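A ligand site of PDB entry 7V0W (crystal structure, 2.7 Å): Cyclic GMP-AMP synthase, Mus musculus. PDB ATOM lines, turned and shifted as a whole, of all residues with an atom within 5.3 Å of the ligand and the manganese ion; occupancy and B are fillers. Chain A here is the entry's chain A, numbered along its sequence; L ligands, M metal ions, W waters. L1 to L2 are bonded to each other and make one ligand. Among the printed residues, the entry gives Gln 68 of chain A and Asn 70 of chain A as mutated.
The side-chain carboxylate of Asp 164 lies within hydrogen-bond range of an oxygen (O5) of LIG L1 (2.5 Å).
The backbone NH (N) of Ser 56 sits close to an oxygen (O5) of LG2 L2, 2.7 Å away.
OG of Ser 56 is in hydrogen-bond range of O2 of LG2 L2 (2.5 Å).
OG of Ser 223 lies within hydrogen-bond range of N4 of LIG L1, at 2.6 Å.
NZ of Lys 207 is in salt-bridge range of O1 of LIG L1 (3.3 Å).
OG of Ser 277 is in hydrogen-bond range of O3 of LG2 L2 (2.9 Å).
O11 of LG2 L2 lies within hydrogen-bond range of SG of Cys 276, 3.0 Å away.
The side-chain amino group (NZ) of Lys 259 is in salt-bridge range of an oxygen (O2) of LG2 L2 (3.1 Å).
The guanidinium group (NH2) of Arg 221 lies within hydrogen-bond range of an oxygen (O14) of LG2 L2.
N4 of LIG L1 lies close to OG of Ser 225, 3.3 Å away.
N3 of LIG L1 sits at hydrogen-bond distance from O of Leu 222 (3.3 Å).
The backbone NH (N) of Asp 164 sits at hydrogen-bond distance from the backbone carbonyl oxygen (O) of Phe 69 (2.9 Å).
The backbone NH (N) of Lys 62 lies within hydrogen-bond range of the backbone carbonyl oxygen (O) of Ser 56.
O of Ser 56 sits at hydrogen-bond distance from N of Val 61.
OG of Ser 223 is in hydrogen-bond range of OG of Ser 225 (3.3 Å).
The backbone carbonyl oxygen (O) of Arg 221 sits at hydrogen-bond distance from the backbone NH (N) of Val 205, at 2.7 Å.
NE2 of His 324 sits at hydrogen-bond distance from OH of Tyr 278 (3.3 Å).
OH of Tyr 278 lies within hydrogen-bond range of OE2 of Glu 228 (2.6 Å).
OG of Ser 148 sits close to N of Ala 150 (3.3 Å).
Merely in contact with the ligand: Gly 55 (3.3 Å), Pro 149 (3.4 Å), Ile 166 (3.5 Å), Tyr 278 (3.5 Å), Val 205 (3.7 Å), Lys 62 (3.9 Å), Ser 148 (3.9 Å), Met 72 (3.9 Å) and Ala 150 (3.98 Å).
Hydrophobic or aromatic side chains within 4 Å of the ligand: Met 72, Pro 149, Ala 150, Ile 166, Val 205 and Tyr 278.
Of the 31 residues printed, 21 come within 4 Å of the ligand.
The nearest printed residue that does not touch the ligand is Glu 59 (4.1 Å).
Ser 56 touches the manganese ion (OG to MN, 3.7 Å).
The nearest printed residue that does not touch the manganese ion is Gly 55 (4.8 Å).
The manganese ion is bound by an oxygen (O1) of LG2 L2 (2.0 Å).
O9 of LG2 L2 binds the manganese ion.
OE1 of Gln 68 binds the manganese ion (2.3 Å).
The manganese ion is bound by water W1 (2.3 Å).
OD1 of Asn 70 is bound to the manganese ion (2.3 Å).
The manganese ion is bound by an oxygen (O5) of LG2 L2 (2.3 Å).
The manganese ion has six donor atoms within binding distance.
Water W1 lies within hydrogen-bond range of the side-chain hydroxyl (OG) of Ser 56 (2.7 Å) and the backbone carbonyl oxygen (O) of Gln 68 (2.7 Å).
Water W3 lies within hydrogen-bond range of O6 of LG2 L2 (2.5 Å), OE1 of Glu 59 (3.0 Å) and NZ of Lys 259 (3.1 Å).
Water W4 lies within hydrogen-bond range of an oxygen (O2) of LG2 L2 and the side-chain amino group of Lys 62.
Water W2 lies within hydrogen-bond range of O6 of LG2 L2, OG of Ser 277 and N of Tyr 278.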
ATOM      1  N   GLY A  55     -17.985  19.049  27.450  1.00  0.00           N
ATOM      2  CA  GLY A  55     -16.807  19.857  27.581  1.00  0.00           C
ATOM      3  C   GLY A  55     -16.104  19.620  28.892  1.00  0.00           C
ATOM      4  O   GLY A  55     -16.492  18.723  29.656  1.00  0.00           O
ATOM      5  N   SER A  56     -15.113  20.478  29.156  1.00  0.00           N
ATOM      6  CA  SER A  56     -14.081  20.202  30.125  1.00  0.00           C
ATOM      7  C   SER A  56     -14.614  20.157  31.541  1.00  0.00           C
ATOM      8  O   SER A  56     -14.152  19.355  32.330  1.00  0.00           O
ATOM      9  CB  SER A  56     -12.876  21.171  29.981  1.00  0.00           C
ATOM     10  OG  SER A  56     -13.219  22.538  30.128  1.00  0.00           O
ATOM     11  N   TYR A  57     -15.585  21.014  31.881  1.00  0.00           N
ATOM     12  CA  TYR A  57     -16.116  21.078  33.270  1.00  0.00           C
ATOM     13  C   TYR A  57     -16.729  19.716  33.638  1.00  0.00           C
ATOM     14  O   TYR A  57     -16.526  19.257  34.764  1.00  0.00           O
ATOM     15  CB  TYR A  57     -17.152  22.186  33.452  1.00  0.00           C
ATOM     16  CG  TYR A  57     -17.869  22.138  34.775  1.00  0.00           C
ATOM     17  CD1 TYR A  57     -17.357  22.731  35.912  1.00  0.00           C
ATOM     18  CD2 TYR A  57     -19.097  21.500  34.898  1.00  0.00           C
ATOM     19  CE1 TYR A  57     -18.030  22.698  37.121  1.00  0.00           C
ATOM     20  CE2 TYR A  57     -19.802  21.457  36.095  1.00  0.00           C
ATOM     21  CZ  TYR A  57     -19.265  22.060  37.220  1.00  0.00           C
ATOM     22  OH  TYR A  57     -19.929  22.046  38.405  1.00  0.00           O
ATOM     23  N   GLU A  59     -16.143  16.860  32.053  1.00  0.00           N
ATOM     24  CA  GLU A  59     -15.094  15.852  31.888  1.00  0.00           C
ATOM     25  C   GLU A  59     -14.069  15.865  33.043  1.00  0.00           C
ATOM     26  O   GLU A  59     -13.182  15.025  33.113  1.00  0.00           O
ATOM     27  CB  GLU A  59     -14.364  16.064  30.560  1.00  0.00           C
ATOM     28  CG  GLU A  59     -15.220  15.880  29.312  1.00  0.00           C
ATOM     29  CD  GLU A  59     -14.622  16.486  28.022  1.00  0.00           C
ATOM     30  OE1 GLU A  59     -13.739  17.383  28.053  1.00  0.00           O
ATOM     31  OE2 GLU A  59     -15.080  16.055  26.945  1.00  0.00           O
ATOM     32  N   VAL A  61     -11.697  18.101  33.449  1.00  0.00           N
ATOM     33  CA  VAL A  61     -10.398  18.602  33.003  1.00  0.00           C
ATOM     34  C   VAL A  61     -10.381  20.129  32.820  1.00  0.00           C
ATOM     35  O   VAL A  61      -9.502  20.682  32.151  1.00  0.00           O
ATOM     36  CB  VAL A  61      -9.928  17.870  31.725  1.00  0.00           C
ATOM     37  CG1 VAL A  61      -9.670  16.405  32.055  1.00  0.00           C
ATOM     38  CG2 VAL A  61     -10.945  17.979  30.592  1.00  0.00           C
ATOM     39  N   LYS A  62     -11.349  20.812  33.427  1.00  0.00           N
ATOM     40  CA  LYS A  62     -11.385  22.247  33.417  1.00  0.00           C
ATOM     41  C   LYS A  62     -10.352  22.738  34.414  1.00  0.00           C
ATOM     42  O   LYS A  62     -10.310  22.275  35.550  1.00  0.00           O
ATOM     43  CB  LYS A  62     -12.766  22.738  33.806  1.00  0.00           C
ATOM     44  CG  LYS A  62     -12.918  24.249  33.857  1.00  0.00           C
ATOM     45  CD  LYS A  62     -13.072  24.838  32.463  1.00  0.00           C
ATOM     46  CE  LYS A  62     -13.053  26.367  32.521  1.00  0.00           C
ATOM     47  NZ  LYS A  62     -11.733  26.946  32.882  1.00  0.00           N
ATOM     48  N   GLN A  68     -16.172  28.583  32.448  1.00  0.00           N
ATOM     49  CA  GLN A  68     -16.600  28.261  31.112  1.00  0.00           C
ATOM     50  C   GLN A  68     -17.252  26.878  31.059  1.00  0.00           C
ATOM     51  O   GLN A  68     -16.662  25.885  31.467  1.00  0.00           O
ATOM     52  CB  GLN A  68     -15.414  28.373  30.162  1.00  0.00           C
ATOM     53  CG  GLN A  68     -15.806  28.724  28.743  1.00  0.00           C
ATOM     54  CD  GLN A  68     -16.280  27.517  27.969  1.00  0.00           C
ATOM     55  OE1 GLN A  68     -16.068  26.397  28.364  1.00  0.00           O
ATOM     56  NE2 GLN A  68     -16.942  27.762  26.867  1.00  0.00           N
ATOM     57  N   PHE A  69     -18.500  26.835  30.555  1.00  0.00           N
ATOM     58  CA  PHE A  69     -19.369  25.652  30.549  1.00  0.00           C
ATOM     59  C   PHE A  69     -19.923  25.433  29.128  1.00  0.00           C
ATOM     60  O   PHE A  69     -20.289  26.375  28.434  1.00  0.00           O
ATOM     61  CB  PHE A  69     -20.578  25.850  31.502  1.00  0.00           C
ATOM     62  CG  PHE A  69     -20.206  25.966  32.970  1.00  0.00           C
ATOM     63  CD1 PHE A  69     -19.690  27.161  33.478  1.00  0.00           C
ATOM     64  CD2 PHE A  69     -20.396  24.891  33.833  1.00  0.00           C
ATOM     65  CE1 PHE A  69     -19.363  27.269  34.823  1.00  0.00           C
ATOM     66  CE2 PHE A  69     -20.055  25.009  35.174  1.00  0.00           C
ATOM     67  CZ  PHE A  69     -19.533  26.177  35.663  1.00  0.00           C
ATOM     68  N   ASN A  70     -19.991  24.167  28.713  1.00  0.00           N
ATOM     69  CA  ASN A  70     -20.601  23.790  27.440  1.00  0.00           C
ATOM     70  C   ASN A  70     -21.836  22.943  27.652  1.00  0.00           C
ATOM     71  O   ASN A  70     -21.768  21.934  28.332  1.00  0.00           O
ATOM     72  CB  ASN A  70     -19.599  23.071  26.578  1.00  0.00           C
ATOM     73  CG  ASN A  70     -18.269  23.795  26.545  1.00  0.00           C
ATOM     74  OD1 ASN A  70     -17.455  23.635  27.443  1.00  0.00           O
ATOM     75  ND2 ASN A  70     -18.062  24.606  25.540  1.00  0.00           N
ATOM     76  N   MET A  72     -25.211  21.322  25.388  1.00  0.00           N
ATOM     77  CA  MET A  72     -25.914  21.085  24.141  1.00  0.00           C
ATOM     78  C   MET A  72     -27.398  21.004  24.424  1.00  0.00           C
ATOM     79  O   MET A  72     -27.815  20.334  25.346  1.00  0.00           O
ATOM     80  CB  MET A  72     -25.409  19.820  23.439  1.00  0.00           C
ATOM     81  CG  MET A  72     -23.928  19.935  23.101  1.00  0.00           C
ATOM     82  SD  MET A  72     -23.120  18.608  22.184  1.00  0.00           S
ATOM     83  CE  MET A  72     -24.274  18.340  20.829  1.00  0.00           C
ATOM     84  N   GLY A 147     -19.911  31.757  12.108  1.00  0.00           N
ATOM     85  CA  GLY A 147     -19.609  30.329  12.103  1.00  0.00           C
ATOM     86  C   GLY A 147     -19.194  29.699  13.442  1.00  0.00           C
ATOM     87  O   GLY A 147     -18.415  28.737  13.462  1.00  0.00           O
ATOM     88  N   SER A 148     -19.694  30.253  14.552  1.00  0.00           N
ATOM     89  CA  SER A 148     -19.739  29.545  15.820  1.00  0.00           C
ATOM     90  C   SER A 148     -21.139  28.959  15.927  1.00  0.00           C
ATOM     91  O   SER A 148     -22.116  29.593  15.567  1.00  0.00           O
ATOM     92  CB  SER A 148     -19.443  30.465  17.015  1.00  0.00           C
ATOM     93  OG  SER A 148     -19.580  29.780  18.245  1.00  0.00           O
ATOM     94  N   PRO A 149     -21.290  27.705  16.399  1.00  0.00           N
ATOM     95  CA  PRO A 149     -22.615  27.143  16.654  1.00  0.00           C
ATOM     96  C   PRO A 149     -23.244  27.588  17.987  1.00  0.00           C
ATOM     97  O   PRO A 149     -24.405  27.246  18.241  1.00  0.00           O
ATOM     98  CB  PRO A 149     -22.284  25.650  16.689  1.00  0.00           C
ATOM     99  CG  PRO A 149     -20.915  25.611  17.337  1.00  0.00           C
ATOM    100  CD  PRO A 149     -20.194  26.775  16.699  1.00  0.00           C
ATOM    101  N   ALA A 150     -22.485  28.323  18.812  1.00  0.00           N
ATOM    102  CA  ALA A 150     -22.865  28.627  20.182  1.00  0.00           C
ATOM    103  C   ALA A 150     -23.653  29.905  20.281  1.00  0.00           C
ATOM    104  O   ALA A 150     -23.478  30.798  19.471  1.00  0.00           O
ATOM    105  CB  ALA A 150     -21.630  28.734  21.054  1.00  0.00           C
ATOM    106  N   ASP A 164     -21.625  28.400  26.861  1.00  0.00           N
ATOM    107  CA  ASP A 164     -21.954  28.213  25.467  1.00  0.00           C
ATOM    108  C   ASP A 164     -23.114  27.257  25.366  1.00  0.00           C
ATOM    109  O   ASP A 164     -23.019  26.133  25.827  1.00  0.00           O
ATOM    110  CB  ASP A 164     -20.737  27.667  24.721  1.00  0.00           C
ATOM    111  CG  ASP A 164     -19.641  28.709  24.585  1.00  0.00           C
ATOM    112  OD1 ASP A 164     -19.955  29.899  24.722  1.00  0.00           O
ATOM    113  OD2 ASP A 164     -18.474  28.332  24.344  1.00  0.00           O
ATOM    114  N   ILE A 166     -25.270  25.275  22.825  1.00  0.00           N
ATOM    115  CA  ILE A 166     -25.032  24.776  21.492  1.00  0.00           C
ATOM    116  C   ILE A 166     -26.264  23.997  21.040  1.00  0.00           C
ATOM    117  O   ILE A 166     -26.598  22.995  21.629  1.00  0.00           O
ATOM    118  CB  ILE A 166     -23.777  23.886  21.476  1.00  0.00           C
ATOM    119  CG1 ILE A 166     -22.583  24.651  22.065  1.00  0.00           C
ATOM    120  CG2 ILE A 166     -23.451  23.441  20.075  1.00  0.00           C
ATOM    121  CD1 ILE A 166     -21.715  23.790  22.962  1.00  0.00           C
ATOM    122  N   VAL A 205     -24.265  20.168  14.620  1.00  0.00           N
ATOM    123  CA  VAL A 205     -24.368  21.482  15.193  1.00  0.00           C
ATOM    124  C   VAL A 205     -24.224  22.496  14.068  1.00  0.00           C
ATOM    125  O   VAL A 205     -23.605  22.205  13.037  1.00  0.00           O
ATOM    126  CB  VAL A 205     -23.322  21.704  16.307  1.00  0.00           C
ATOM    127  CG1 VAL A 205     -23.623  20.773  17.496  1.00  0.00           C
ATOM    128  CG2 VAL A 205     -21.897  21.524  15.776  1.00  0.00           C
ATOM    129  N   LYS A 207     -22.358  24.809  12.864  1.00  0.00           N
ATOM    130  CA  LYS A 207     -21.102  25.458  12.589  1.00  0.00           C
ATOM    131  C   LYS A 207     -21.070  25.417  11.089  1.00  0.00           C
ATOM    132  O   LYS A 207     -21.238  24.374  10.496  1.00  0.00           O
ATOM    133  CB  LYS A 207     -19.896  24.707  13.209  1.00  0.00           C
ATOM    134  CG  LYS A 207     -18.553  25.447  13.129  1.00  0.00           C
ATOM    135  CD  LYS A 207     -17.605  25.147  14.309  1.00  0.00           C
ATOM    136  CE  LYS A 207     -16.988  23.761  14.182  1.00  0.00           C
ATOM    137  NZ  LYS A 207     -16.568  22.993  15.398  1.00  0.00           N
ATOM    138  N   ARG A 221     -22.349  20.644  11.141  1.00  0.00           N
ATOM    139  CA  ARG A 221     -21.085  19.932  11.473  1.00  0.00           C
ATOM    140  C   ARG A 221     -21.343  18.804  12.474  1.00  0.00           C
ATOM    141  O   ARG A 221     -22.142  19.035  13.415  1.00  0.00           O
ATOM    142  CB  ARG A 221     -20.041  20.878  12.064  1.00  0.00           C
ATOM    143  CG  ARG A 221     -18.621  20.348  11.944  1.00  0.00           C
ATOM    144  CD  ARG A 221     -17.684  21.222  12.744  1.00  0.00           C
ATOM    145  NE  ARG A 221     -16.341  20.701  12.913  1.00  0.00           N
ATOM    146  CZ  ARG A 221     -16.035  19.608  13.603  1.00  0.00           C
ATOM    147  NH1 ARG A 221     -16.975  18.877  14.172  1.00  0.00           N
ATOM    148  NH2 ARG A 221     -14.760  19.232  13.718  1.00  0.00           N
ATOM    149  N   LEU A 222     -20.658  17.672  12.279  1.00  0.00           N
ATOM    150  CA  LEU A 222     -20.757  16.523  13.173  1.00  0.00           C
ATOM    151  C   LEU A 222     -20.241  16.847  14.543  1.00  0.00           C
ATOM    152  O   LEU A 222     -19.282  17.577  14.677  1.00  0.00           O
ATOM    153  CB  LEU A 222     -19.960  15.348  12.621  1.00  0.00           C
ATOM    154  CG  LEU A 222     -20.561  14.621  11.426  1.00  0.00           C
ATOM    155  CD1 LEU A 222     -19.572  13.615  10.875  1.00  0.00           C
ATOM    156  CD2 LEU A 222     -21.869  13.969  11.817  1.00  0.00           C
ATOM    157  N   SER A 223     -20.888  16.288  15.576  1.00  0.00           N
ATOM    158  CA  SER A 223     -20.445  16.381  16.956  1.00  0.00           C
ATOM    159  C   SER A 223     -20.430  15.019  17.641  1.00  0.00           C
ATOM    160  O   SER A 223     -21.376  14.231  17.534  1.00  0.00           O
ATOM    161  CB  SER A 223     -21.317  17.357  17.767  1.00  0.00           C
ATOM    162  OG  SER A 223     -20.850  17.451  19.133  1.00  0.00           O
ATOM    163  N   PHE A 224     -19.327  14.766  18.353  1.00  0.00           N
ATOM    164  CA  PHE A 224     -19.149  13.617  19.220  1.00  0.00           C
ATOM    165  C   PHE A 224     -18.716  14.071  20.604  1.00  0.00           C
ATOM    166  O   PHE A 224     -17.870  13.453  21.209  1.00  0.00           O
ATOM    167  CB  PHE A 224     -18.090  12.684  18.615  1.00  0.00           C
ATOM    168  CG  PHE A 224     -18.326  12.415  17.162  1.00  0.00           C
ATOM    169  CD1 PHE A 224     -19.195  11.422  16.763  1.00  0.00           C
ATOM    170  CD2 PHE A 224     -17.746  13.221  16.230  1.00  0.00           C
ATOM    171  CE1 PHE A 224     -19.435  11.216  15.429  1.00  0.00           C
ATOM    172  CE2 PHE A 224     -17.991  13.023  14.876  1.00  0.00           C
ATOM    173  CZ  PHE A 224     -18.823  12.011  14.481  1.00  0.00           C
ATOM    174  N   SER A 225     -19.290  15.174  21.090  1.00  0.00           N
ATOM    175  CA  SER A 225     -18.988  15.689  22.417  1.00  0.00           C
ATOM    176  C   SER A 225     -19.411  14.697  23.488  1.00  0.00           C
ATOM    177  O   SER A 225     -18.754  14.583  24.514  1.00  0.00           O
ATOM    178  CB  SER A 225     -19.719  16.996  22.661  1.00  0.00           C
ATOM    179  OG  SER A 225     -19.140  18.027  21.906  1.00  0.00           O
ATOM    180  N   GLU A 228     -16.757  11.906  23.425  1.00  0.00           N
ATOM    181  CA  GLU A 228     -15.559  12.419  24.036  1.00  0.00           C
ATOM    182  C   GLU A 228     -15.675  12.440  25.573  1.00  0.00           C
ATOM    183  O   GLU A 228     -14.694  12.166  26.289  1.00  0.00           O
ATOM    184  CB  GLU A 228     -15.295  13.807  23.476  1.00  0.00           C
ATOM    185  CG  GLU A 228     -14.911  13.800  21.992  1.00  0.00           C
ATOM    186  CD  GLU A 228     -15.074  15.124  21.310  1.00  0.00           C
ATOM    187  OE1 GLU A 228     -15.228  16.138  22.027  1.00  0.00           O
ATOM    188  OE2 GLU A 228     -15.044  15.151  20.052  1.00  0.00           O
ATOM    189  N   LYS A 259      -3.417  21.787  28.124  1.00  0.00           N
ATOM    190  CA  LYS A 259      -4.401  22.842  27.920  1.00  0.00           C
ATOM    191  C   LYS A 259      -3.909  24.163  28.454  1.00  0.00           C
ATOM    192  O   LYS A 259      -4.093  25.199  27.819  1.00  0.00           O
ATOM    193  CB  LYS A 259      -5.696  22.521  28.626  1.00  0.00           C
ATOM    194  CG  LYS A 259      -6.515  21.478  27.918  1.00  0.00           C
ATOM    195  CD  LYS A 259      -7.490  20.887  28.919  1.00  0.00           C
ATOM    196  CE  LYS A 259      -8.594  21.864  29.299  1.00  0.00           C
ATOM    197  NZ  LYS A 259      -9.817  21.506  28.528  1.00  0.00           N
ATOM    198  N   GLU A 263      -3.439  27.751  26.785  1.00  0.00           N
ATOM    199  CA  GLU A 263      -4.134  28.916  27.337  1.00  0.00           C
ATOM    200  C   GLU A 263      -3.154  30.076  27.648  1.00  0.00           C
ATOM    201  O   GLU A 263      -3.387  31.235  27.250  1.00  0.00           O
ATOM    202  CB  GLU A 263      -4.932  28.574  28.614  1.00  0.00           C
ATOM    203  CG  GLU A 263      -6.343  28.072  28.354  1.00  0.00           C
ATOM    204  CD  GLU A 263      -7.141  27.815  29.638  1.00  0.00           C
ATOM    205  OE1 GLU A 263      -7.069  28.667  30.564  1.00  0.00           O
ATOM    206  OE2 GLU A 263      -7.846  26.751  29.716  1.00  0.00           O
ATOM    207  N   CYS A 276      -6.758  26.052  19.383  1.00  0.00           N
ATOM    208  CA  CYS A 276      -7.796  25.941  20.393  1.00  0.00           C
ATOM    209  C   CYS A 276      -7.565  24.668  21.187  1.00  0.00           C
ATOM    210  O   CYS A 276      -6.704  23.881  20.865  1.00  0.00           O
ATOM    211  CB  CYS A 276      -9.178  25.922  19.732  1.00  0.00           C
ATOM    212  SG  CYS A 276      -9.433  24.469  18.700  1.00  0.00           S
ATOM    213  N   SER A 277      -8.352  24.467  22.243  1.00  0.00           N
ATOM    214  CA  SER A 277      -8.104  23.360  23.132  1.00  0.00           C
ATOM    215  C   SER A 277      -8.513  22.039  22.477  1.00  0.00           C
ATOM    216  O   SER A 277      -8.035  20.974  22.874  1.00  0.00           O
ATOM    217  CB  SER A 277      -8.778  23.574  24.492  1.00  0.00           C
ATOM    218  OG  SER A 277     -10.183  23.729  24.365  1.00  0.00           O
ATOM    219  N   TYR A 278      -9.413  22.089  21.486  1.00  0.00           N
ATOM    220  CA  TYR A 278      -9.881  20.874  20.787  1.00  0.00           C
ATOM    221  C   TYR A 278      -8.686  20.194  20.087  1.00  0.00           C
ATOM    222  O   TYR A 278      -8.671  18.943  19.949  1.00  0.00           O
ATOM    223  CB  TYR A 278     -11.008  21.163  19.776  1.00  0.00           C
ATOM    224  CG  TYR A 278     -11.667  19.876  19.352  1.00  0.00           C
ATOM    225  CD1 TYR A 278     -12.445  19.175  20.257  1.00  0.00           C
ATOM    226  CD2 TYR A 278     -11.420  19.308  18.105  1.00  0.00           C
ATOM    227  CE1 TYR A 278     -13.034  17.964  19.909  1.00  0.00           C
ATOM    228  CE2 TYR A 278     -11.982  18.079  17.759  1.00  0.00           C
ATOM    229  CZ  TYR A 278     -12.775  17.411  18.672  1.00  0.00           C
ATOM    230  OH  TYR A 278     -13.346  16.212  18.366  1.00  0.00           O
ATOM    231  N   LYS A 281      -6.916  18.246  22.814  1.00  0.00           N
ATOM    232  CA  LYS A 281      -7.787  17.100  23.125  1.00  0.00           C
ATOM    233  C   LYS A 281      -7.682  16.001  22.071  1.00  0.00           C
ATOM    234  O   LYS A 281      -7.567  14.827  22.400  1.00  0.00           O
ATOM    235  CB  LYS A 281      -9.229  17.569  23.218  1.00  0.00           C
ATOM    236  CG  LYS A 281     -10.137  16.645  23.979  1.00  0.00           C
ATOM    237  CD  LYS A 281     -11.528  17.243  23.967  1.00  0.00           C
ATOM    238  CE  LYS A 281     -12.364  16.629  25.040  1.00  0.00           C
ATOM    239  NZ  LYS A 281     -13.783  16.496  24.601  1.00  0.00           N
ATOM    240  N   HIS A 324      -8.713  14.473  12.805  1.00  0.00           N
ATOM    241  CA  HIS A 324      -9.879  14.345  13.678  1.00  0.00           C
ATOM    242  C   HIS A 324      -9.947  12.910  14.120  1.00  0.00           C
ATOM    243  O   HIS A 324      -9.761  12.001  13.317  1.00  0.00           O
ATOM    244  CB  HIS A 324     -11.185  14.732  12.949  1.00  0.00           C
ATOM    245  CG  HIS A 324     -12.309  15.103  13.865  1.00  0.00           C
ATOM    246  ND1 HIS A 324     -13.049  14.161  14.533  1.00  0.00           N
ATOM    247  CD2 HIS A 324     -12.803  16.307  14.222  1.00  0.00           C
ATOM    248  CE1 HIS A 324     -13.965  14.771  15.270  1.00  0.00           C
ATOM    249  NE2 HIS A 324     -13.841  16.073  15.102  1.00  0.00           N
HETATM  250  P1  LIG L   1     -15.473  26.872  17.833  1.00  0.00           P
HETATM  251  O1  LIG L   1     -15.357  25.670  16.920  1.00  0.00           O
HETATM  252  O2  LIG L   1     -15.579  28.208  17.148  1.00  0.00           O
HETATM  253  O3  LIG L   1     -16.758  26.667  18.790  1.00  0.00           O
HETATM  254  C1  LIG L   1     -16.969  27.507  19.944  1.00  0.00           C
HETATM  255  C2  LIG L   1     -18.097  26.934  20.758  1.00  0.00           C
HETATM  256  O4  LIG L   1     -18.822  25.980  19.942  1.00  0.00           O
HETATM  257  C3  LIG L   1     -17.699  26.152  22.019  1.00  0.00           C
HETATM  258  O5  LIG L   1     -18.687  26.270  23.035  1.00  0.00           O
HETATM  259  C4  LIG L   1     -17.640  24.712  21.510  1.00  0.00           C
HETATM  260  O6  LIG L   1     -17.826  23.737  22.506  1.00  0.00           O
HETATM  261  C5  LIG L   1     -18.822  24.715  20.559  1.00  0.00           C
HETATM  262  N1  LIG L   1     -18.719  23.675  19.547  1.00  0.00           N
HETATM  263  C6  LIG L   1     -18.057  23.744  18.337  1.00  0.00           C
HETATM  264  N2  LIG L   1     -18.145  22.624  17.650  1.00  0.00           N
HETATM  265  C7  LIG L   1     -18.894  21.786  18.471  1.00  0.00           C
HETATM  266  C8  LIG L   1     -19.318  20.446  18.308  1.00  0.00           C
HETATM  267  N3  LIG L   1     -19.045  19.727  17.234  1.00  0.00           N
HETATM  268  N4  LIG L   1     -20.050  19.904  19.313  1.00  0.00           N
HETATM  269  C9  LIG L   1     -20.314  20.654  20.389  1.00  0.00           C
HETATM  270  N5  LIG L   1     -19.969  21.917  20.647  1.00  0.00           N
HETATM  271  C10 LIG L   1     -19.246  22.419  19.637  1.00  0.00           C
HETATM  272  P1  LG2 L   2     -11.985  24.281  27.600  1.00  0.00           P
HETATM  273  O1  LG2 L   2     -13.369  24.874  27.544  1.00  0.00           O
HETATM  274  O2  LG2 L   2     -11.521  24.045  29.024  1.00  0.00           O
HETATM  275  O3  LG2 L   2     -10.990  25.059  26.778  1.00  0.00           O
HETATM  276  O4  LG2 L   2     -12.108  22.829  26.909  1.00  0.00           O
HETATM  277  P2  LG2 L   2     -13.373  22.080  26.263  1.00  0.00           P
HETATM  278  O5  LG2 L   2     -14.544  22.262  27.156  1.00  0.00           O
HETATM  279  O6  LG2 L   2     -12.979  20.693  25.839  1.00  0.00           O
HETATM  280  O7  LG2 L   2     -13.544  22.970  24.948  1.00  0.00           O
HETATM  281  P3  LG2 L   2     -14.687  23.950  24.381  1.00  0.00           P
HETATM  282  O8  LG2 L   2     -15.647  23.169  23.553  1.00  0.00           O
HETATM  283  O9  LG2 L   2     -15.196  24.738  25.537  1.00  0.00           O
HETATM  284  O10 LG2 L   2     -13.833  24.900  23.419  1.00  0.00           O
HETATM  285  C1  LG2 L   2     -12.950  24.235  22.479  1.00  0.00           C
HETATM  286  C2  LG2 L   2     -12.383  25.230  21.491  1.00  0.00           C
HETATM  287  O11 LG2 L   2     -11.993  24.518  20.286  1.00  0.00           O
HETATM  288  C3  LG2 L   2     -13.328  26.350  21.024  1.00  0.00           C
HETATM  289  O12 LG2 L   2     -12.554  27.529  20.841  1.00  0.00           O
HETATM  290  C4  LG2 L   2     -13.909  25.791  19.728  1.00  0.00           C
HETATM  291  O13 LG2 L   2     -14.244  26.911  18.876  1.00  0.00           O
HETATM  292  C5  LG2 L   2     -12.750  24.957  19.183  1.00  0.00           C
HETATM  293  N1  LG2 L   2     -13.142  23.767  18.383  1.00  0.00           N
HETATM  294  C6  LG2 L   2     -12.742  23.506  17.087  1.00  0.00           C
HETATM  295  N2  LG2 L   2     -13.251  22.396  16.611  1.00  0.00           N
HETATM  296  C7  LG2 L   2     -14.029  21.902  17.654  1.00  0.00           C
HETATM  297  C8  LG2 L   2     -14.817  20.717  17.722  1.00  0.00           C
HETATM  298  O14 LG2 L   2     -14.982  19.863  16.847  1.00  0.00           O
HETATM  299  N3  LG2 L   2     -15.446  20.596  18.966  1.00  0.00           N
HETATM  300  C9  LG2 L   2     -15.323  21.480  20.005  1.00  0.00           C
HETATM  301  N4  LG2 L   2     -16.007  21.191  21.122  1.00  0.00           N
HETATM  302  N5  LG2 L   2     -14.578  22.591  19.954  1.00  0.00           N
HETATM  303  C10 LG2 L   2     -13.970  22.735  18.745  1.00  0.00           C
HETATM  304 MN    MN M   1     -15.295  24.388  27.691  1.00  0.00          MN
HETATM  305  O   HOH W   1     -15.518  23.925  29.914  1.00  0.00           O
HETATM  306  O   HOH W   2     -11.055  20.942  24.017  1.00  0.00           O
HETATM  307  O   HOH W   3     -11.505  19.214  27.267  1.00  0.00           O
HETATM  308  O   HOH W   4     -10.215  24.534  31.258  1.00  0.00           O
